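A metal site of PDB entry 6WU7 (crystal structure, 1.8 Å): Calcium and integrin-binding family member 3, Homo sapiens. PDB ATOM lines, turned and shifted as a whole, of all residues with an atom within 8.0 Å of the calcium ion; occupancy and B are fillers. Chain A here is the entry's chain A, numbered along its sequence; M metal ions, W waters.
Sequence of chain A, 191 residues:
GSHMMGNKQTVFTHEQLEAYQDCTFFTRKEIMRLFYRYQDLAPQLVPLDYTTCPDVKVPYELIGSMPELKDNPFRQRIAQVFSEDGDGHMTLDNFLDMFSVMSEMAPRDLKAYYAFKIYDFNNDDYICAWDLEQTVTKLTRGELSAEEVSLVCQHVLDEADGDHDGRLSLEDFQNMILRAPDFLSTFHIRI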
ATOM      1  N   PHE A 116     -31.052  -0.466  29.382  1.00  0.00           N
ATOM      2  CA  PHE A 116     -30.413   0.753  28.886  1.00  0.00           C
ATOM      3  C   PHE A 116     -29.420   0.438  27.777  1.00  0.00           C
ATOM      4  O   PHE A 116     -29.429   1.075  26.713  1.00  0.00           O
ATOM      5  CB  PHE A 116     -29.707   1.494  30.018  1.00  0.00           C
ATOM      6  CG  PHE A 116     -29.076   2.782  29.568  1.00  0.00           C
ATOM      7  CD1 PHE A 116     -29.843   3.917  29.472  1.00  0.00           C
ATOM      8  CD2 PHE A 116     -27.725   2.829  29.247  1.00  0.00           C
ATOM      9  CE1 PHE A 116     -29.276   5.119  29.054  1.00  0.00           C
ATOM     10  CE2 PHE A 116     -27.157   4.040  28.819  1.00  0.00           C
ATOM     11  CZ  PHE A 116     -27.935   5.158  28.726  1.00  0.00           C
ATOM     12  N   LYS A 117     -28.543  -0.554  27.994  1.00  0.00           N
ATOM     13  CA  LYS A 117     -27.548  -0.900  26.992  1.00  0.00           C
ATOM     14  C   LYS A 117     -28.219  -1.338  25.700  1.00  0.00           C
ATOM     15  O   LYS A 117     -27.749  -1.017  24.604  1.00  0.00           O
ATOM     16  CB  LYS A 117     -26.630  -2.018  27.510  1.00  0.00           C
ATOM     17  CG  LYS A 117     -25.973  -1.671  28.833  1.00  0.00           C
ATOM     18  CD  LYS A 117     -24.636  -2.364  29.125  1.00  0.00           C
ATOM     19  CE  LYS A 117     -24.425  -3.640  28.324  1.00  0.00           C
ATOM     20  NZ  LYS A 117     -23.138  -4.313  28.644  1.00  0.00           N
ATOM     21  N   TYR A 119     -31.328  -0.637  24.573  1.00  0.00           N
ATOM     22  CA  TYR A 119     -32.062   0.442  23.936  1.00  0.00           C
ATOM     23  C   TYR A 119     -31.181   1.598  23.446  1.00  0.00           C
ATOM     24  O   TYR A 119     -31.675   2.474  22.720  1.00  0.00           O
ATOM     25  CB  TYR A 119     -33.091   0.977  24.921  1.00  0.00           C
ATOM     26  CG  TYR A 119     -34.172  -0.017  25.295  1.00  0.00           C
ATOM     27  CD1 TYR A 119     -34.557  -1.042  24.440  1.00  0.00           C
ATOM     28  CD2 TYR A 119     -34.837   0.098  26.507  1.00  0.00           C
ATOM     29  CE1 TYR A 119     -35.561  -1.923  24.777  1.00  0.00           C
ATOM     30  CE2 TYR A 119     -35.855  -0.763  26.844  1.00  0.00           C
ATOM     31  CZ  TYR A 119     -36.224  -1.786  25.992  1.00  0.00           C
ATOM     32  OH  TYR A 119     -37.239  -2.661  26.325  1.00  0.00           O
ATOM     33  N   ASP A 120     -29.922   1.637  23.868  1.00  0.00           N
ATOM     34  CA  ASP A 120     -28.953   2.621  23.402  1.00  0.00           C
ATOM     35  C   ASP A 120     -28.403   2.102  22.074  1.00  0.00           C
ATOM     36  O   ASP A 120     -27.297   1.568  21.973  1.00  0.00           O
ATOM     37  CB  ASP A 120     -27.878   2.824  24.464  1.00  0.00           C
ATOM     38  CG  ASP A 120     -26.695   3.603  23.957  1.00  0.00           C
ATOM     39  OD1 ASP A 120     -26.826   4.328  22.952  1.00  0.00           O
ATOM     40  OD2 ASP A 120     -25.627   3.503  24.591  1.00  0.00           O
ATOM     41  N   PHE A 121     -29.225   2.256  21.030  1.00  0.00           N
ATOM     42  CA  PHE A 121     -28.993   1.567  19.773  1.00  0.00           C
ATOM     43  C   PHE A 121     -27.631   1.919  19.157  1.00  0.00           C
ATOM     44  O   PHE A 121     -27.065   1.111  18.404  1.00  0.00           O
ATOM     45  CB  PHE A 121     -30.129   1.865  18.758  1.00  0.00           C
ATOM     46  CG  PHE A 121     -31.397   1.031  18.975  1.00  0.00           C
ATOM     47  CD1 PHE A 121     -31.611  -0.127  18.243  1.00  0.00           C
ATOM     48  CD2 PHE A 121     -32.364   1.437  19.868  1.00  0.00           C
ATOM     49  CE1 PHE A 121     -32.772  -0.898  18.436  1.00  0.00           C
ATOM     50  CE2 PHE A 121     -33.516   0.664  20.079  1.00  0.00           C
ATOM     51  CZ  PHE A 121     -33.709  -0.492  19.359  1.00  0.00           C
ATOM     52  N   ASN A 122     -27.084   3.110  19.423  1.00  0.00           N
ATOM     53  CA  ASN A 122     -25.808   3.500  18.822  1.00  0.00           C
ATOM     54  C   ASN A 122     -24.646   3.472  19.812  1.00  0.00           C
ATOM     55  O   ASN A 122     -23.544   3.920  19.485  1.00  0.00           O
ATOM     56  CB  ASN A 122     -25.884   4.882  18.163  1.00  0.00           C
ATOM     57  CG  ASN A 122     -26.512   5.942  19.057  1.00  0.00           C
ATOM     58  OD1 ASN A 122     -26.636   5.770  20.267  1.00  0.00           O
ATOM     59  ND2 ASN A 122     -26.905   7.056  18.445  1.00  0.00           N
ATOM     60  N   ASN A 123     -24.867   2.936  21.004  1.00  0.00           N
ATOM     61  CA  ASN A 123     -23.809   2.711  21.988  1.00  0.00           C
ATOM     62  C   ASN A 123     -23.022   3.984  22.302  1.00  0.00           C
ATOM     63  O   ASN A 123     -21.797   3.976  22.375  1.00  0.00           O
ATOM     64  CB  ASN A 123     -22.883   1.586  21.523  1.00  0.00           C
ATOM     65  CG  ASN A 123     -23.640   0.354  21.053  1.00  0.00           C
ATOM     66  OD1 ASN A 123     -24.289  -0.333  21.834  1.00  0.00           O
ATOM     67  ND2 ASN A 123     -23.552   0.072  19.760  1.00  0.00           N
ATOM     68  N   ASP A 124     -23.732   5.090  22.523  1.00  0.00           N
ATOM     69  CA  ASP A 124     -23.053   6.328  22.897  1.00  0.00           C
ATOM     70  C   ASP A 124     -23.345   6.734  24.341  1.00  0.00           C
ATOM     71  O   ASP A 124     -23.043   7.861  24.733  1.00  0.00           O
ATOM     72  CB  ASP A 124     -23.394   7.448  21.911  1.00  0.00           C
ATOM     73  CG  ASP A 124     -24.818   7.970  22.068  1.00  0.00           C
ATOM     74  OD1 ASP A 124     -25.641   7.327  22.727  1.00  0.00           O
ATOM     75  OD2 ASP A 124     -25.073   9.057  21.474  1.00  0.00           O
ATOM     76  N   ASP A 125     -23.912   5.807  25.118  1.00  0.00           N
ATOM     77  CA  ASP A 125     -24.183   5.936  26.563  1.00  0.00           C
ATOM     78  C   ASP A 125     -25.287   6.929  26.888  1.00  0.00           C
ATOM     79  O   ASP A 125     -25.404   7.398  28.016  1.00  0.00           O
ATOM     80  CB  ASP A 125     -22.898   6.275  27.312  1.00  0.00           C
ATOM     81  CG  ASP A 125     -21.802   5.267  27.011  1.00  0.00           C
ATOM     82  OD1 ASP A 125     -22.059   4.062  27.172  1.00  0.00           O
ATOM     83  OD2 ASP A 125     -20.726   5.657  26.589  1.00  0.00           O
ATOM     84  N   TYR A 126     -26.138   7.216  25.920  1.00  0.00           N
ATOM     85  CA  TYR A 126     -27.322   8.018  26.137  1.00  0.00           C
ATOM     86  C   TYR A 126     -28.449   7.398  25.332  1.00  0.00           C
ATOM     87  O   TYR A 126     -28.221   6.853  24.251  1.00  0.00           O
ATOM     88  CB  TYR A 126     -27.151   9.482  25.702  1.00  0.00           C
ATOM     89  CG  TYR A 126     -26.180  10.281  26.518  1.00  0.00           C
ATOM     90  CD1 TYR A 126     -26.564  10.905  27.698  1.00  0.00           C
ATOM     91  CD2 TYR A 126     -24.853  10.431  26.110  1.00  0.00           C
ATOM     92  CE1 TYR A 126     -25.669  11.631  28.441  1.00  0.00           C
ATOM     93  CE2 TYR A 126     -23.956  11.134  26.860  1.00  0.00           C
ATOM     94  CZ  TYR A 126     -24.375  11.740  28.022  1.00  0.00           C
ATOM     95  OH  TYR A 126     -23.500  12.468  28.775  1.00  0.00           O
ATOM     96  N   ILE A 127     -29.653   7.518  25.836  1.00  0.00           N
ATOM     97  CA  ILE A 127     -30.839   7.189  25.062  1.00  0.00           C
ATOM     98  C   ILE A 127     -31.426   8.519  24.629  1.00  0.00           C
ATOM     99  O   ILE A 127     -31.953   9.259  25.456  1.00  0.00           O
ATOM    100  CB  ILE A 127     -31.841   6.344  25.864  1.00  0.00           C
ATOM    101  CG1 ILE A 127     -31.265   4.936  26.045  1.00  0.00           C
ATOM    102  CG2 ILE A 127     -33.163   6.282  25.134  1.00  0.00           C
ATOM    103  CD1 ILE A 127     -32.181   3.998  26.849  1.00  0.00           C
ATOM    104  N   CYS A 128     -31.289   8.835  23.351  1.00  0.00           N
ATOM    105  CA  CYS A 128     -31.769  10.071  22.775  1.00  0.00           C
ATOM    106  C   CYS A 128     -33.191   9.901  22.262  1.00  0.00           C
ATOM    107  O   CYS A 128     -33.803   8.830  22.391  1.00  0.00           O
ATOM    108  CB  CYS A 128     -30.848  10.543  21.652  1.00  0.00           C
ATOM    109  SG  CYS A 128     -30.873   9.459  20.205  1.00  0.00           S
ATOM    110  N   ALA A 129     -33.732  10.951  21.671  1.00  0.00           N
ATOM    111  CA  ALA A 129     -35.073  10.855  21.104  1.00  0.00           C
ATOM    112  C   ALA A 129     -35.152   9.817  19.993  1.00  0.00           C
ATOM    113  O   ALA A 129     -36.200   9.182  19.820  1.00  0.00           O
ATOM    114  CB  ALA A 129     -35.526  12.223  20.586  1.00  0.00           C
ATOM    115  N   TRP A 130     -34.070   9.640  19.205  1.00  0.00           N
ATOM    116  CA  TRP A 130     -34.123   8.622  18.162  1.00  0.00           C
ATOM    117  C   TRP A 130     -34.087   7.231  18.761  1.00  0.00           C
ATOM    118  O   TRP A 130     -34.788   6.322  18.281  1.00  0.00           O
ATOM    119  CB  TRP A 130     -32.965   8.775  17.163  1.00  0.00           C
ATOM    120  CG  TRP A 130     -32.983   7.763  15.991  1.00  0.00           C
ATOM    121  CD1 TRP A 130     -31.891   7.298  15.310  1.00  0.00           C
ATOM    122  CD2 TRP A 130     -34.131   7.137  15.364  1.00  0.00           C
ATOM    123  NE1 TRP A 130     -32.279   6.425  14.306  1.00  0.00           N
ATOM    124  CE2 TRP A 130     -33.650   6.309  14.325  1.00  0.00           C
ATOM    125  CE3 TRP A 130     -35.514   7.186  15.589  1.00  0.00           C
ATOM    126  CZ2 TRP A 130     -34.491   5.542  13.515  1.00  0.00           C
ATOM    127  CZ3 TRP A 130     -36.359   6.420  14.771  1.00  0.00           C
ATOM    128  CH2 TRP A 130     -35.839   5.609  13.759  1.00  0.00           C
ATOM    129  N   ASP A 131     -33.257   7.025  19.806  1.00  0.00           N
ATOM    130  CA  ASP A 131     -33.228   5.716  20.463  1.00  0.00           C
ATOM    131  C   ASP A 131     -34.581   5.417  21.081  1.00  0.00           C
ATOM    132  O   ASP A 131     -35.077   4.283  20.999  1.00  0.00           O
ATOM    133  CB  ASP A 131     -32.151   5.682  21.563  1.00  0.00           C
ATOM    134  CG  ASP A 131     -30.732   5.600  21.023  1.00  0.00           C
ATOM    135  OD1 ASP A 131     -30.565   5.212  19.846  1.00  0.00           O
ATOM    136  OD2 ASP A 131     -29.764   5.931  21.783  1.00  0.00           O
ATOM    137  N   LEU A 132     -35.193   6.418  21.723  1.00  0.00           N
ATOM    138  CA  LEU A 132     -36.517   6.238  22.329  1.00  0.00           C
ATOM    139  C   LEU A 132     -37.561   5.895  21.291  1.00  0.00           C
ATOM    140  O   LEU A 132     -38.414   5.027  21.509  1.00  0.00           O
ATOM    141  CB  LEU A 132     -36.894   7.527  23.058  1.00  0.00           C
ATOM    142  CG  LEU A 132     -37.551   7.454  24.423  1.00  0.00           C
ATOM    143  CD1 LEU A 132     -37.016   6.341  25.257  1.00  0.00           C
ATOM    144  CD2 LEU A 132     -37.368   8.797  25.126  1.00  0.00           C
ATOM    145  N   GLN A 134     -37.207   4.471  18.319  1.00  0.00           N
ATOM    146  CA  GLN A 134     -37.032   3.087  17.893  1.00  0.00           C
ATOM    147  C   GLN A 134     -37.544   2.125  18.943  1.00  0.00           C
ATOM    148  O   GLN A 134     -38.188   1.118  18.624  1.00  0.00           O
ATOM    149  CB  GLN A 134     -35.561   2.789  17.639  1.00  0.00           C
ATOM    150  CG  GLN A 134     -34.943   3.442  16.454  1.00  0.00           C
ATOM    151  CD  GLN A 134     -33.508   2.985  16.310  1.00  0.00           C
ATOM    152  OE1 GLN A 134     -33.240   1.836  15.946  1.00  0.00           O
ATOM    153  NE2 GLN A 134     -32.575   3.877  16.617  1.00  0.00           N
ATOM    154  N   ARG A 167     -31.892  14.112  26.581  1.00  0.00           N
ATOM    155  CA  ARG A 167     -31.612  12.699  26.415  1.00  0.00           C
ATOM    156  C   ARG A 167     -31.428  12.059  27.785  1.00  0.00           C
ATOM    157  O   ARG A 167     -31.267  12.726  28.810  1.00  0.00           O
ATOM    158  CB  ARG A 167     -30.384  12.462  25.535  1.00  0.00           C
ATOM    159  CG  ARG A 167     -29.168  13.173  25.982  1.00  0.00           C
ATOM    160  CD  ARG A 167     -28.099  13.136  24.925  1.00  0.00           C
ATOM    161  NE  ARG A 167     -26.963  13.916  25.386  1.00  0.00           N
ATOM    162  CZ  ARG A 167     -25.736  13.811  24.906  1.00  0.00           C
ATOM    163  NH1 ARG A 167     -25.462  12.969  23.936  1.00  0.00           N
ATOM    164  NH2 ARG A 167     -24.779  14.572  25.421  1.00  0.00           N
ATOM    165  N   LEU A 168     -31.510  10.733  27.788  1.00  0.00           N
ATOM    166  CA  LEU A 168     -31.512   9.967  29.022  1.00  0.00           C
ATOM    167  C   LEU A 168     -30.157   9.332  29.234  1.00  0.00           C
ATOM    168  O   LEU A 168     -29.705   8.530  28.415  1.00  0.00           O
ATOM    169  CB  LEU A 168     -32.573   8.873  28.969  1.00  0.00           C
ATOM    170  CG  LEU A 168     -34.014   9.360  28.838  1.00  0.00           C
ATOM    171  CD1 LEU A 168     -34.909   8.118  28.942  1.00  0.00           C
ATOM    172  CD2 LEU A 168     -34.370  10.414  29.842  1.00  0.00           C
HETATM  173 CA    CA M   1     -27.637   6.394  22.160  1.00  0.00          CA
HETATM  174  O   HOH W   1     -28.218   8.618  21.272  1.00  0.00           O
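The side-chain carboxylate (OD1) of Asp 131 lies within hydrogen-bond range of the backbone NH (N) of Phe 121. The backbone NH (N) of Asp 125 sits at hydrogen-bond distance from the side-chain carboxylate (OD2) of Asp 120 (2.9 Å). The backbone NH (N) of Asp 131 lies within hydrogen-bond range of the side-chain sulfur (SG) of Cys 128. The side-chain carboxylate (OD1) of Asp 120 lies close to the backbone NH (N) of Asn 123 (3.1 Å).
The calcium ion is bound by the side-chain carboxylate of Asp 131, the backbone carbonyl oxygen of Tyr 126, the side-chain amide oxygen of Asn 122, the side-chain carboxylate of Asp 124, the side-chain carboxylate of Asp 120 and water W1. The calcium ion has six donor atoms within binding distance.
Of the 19 residues printed, 5 come within 4 Å of the calcium ion. The nearest printed residue that does not touch the calcium ion is Ile 127 (4.3 Å).
Water W1 lies within hydrogen-bond range of the side-chain sulfur of Cys 128 (3.0 Å), the side-chain carboxylate of Asp 124 (3.2 Å) and the side-chain amide nitrogen of Asn 122 (3.5 Å).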
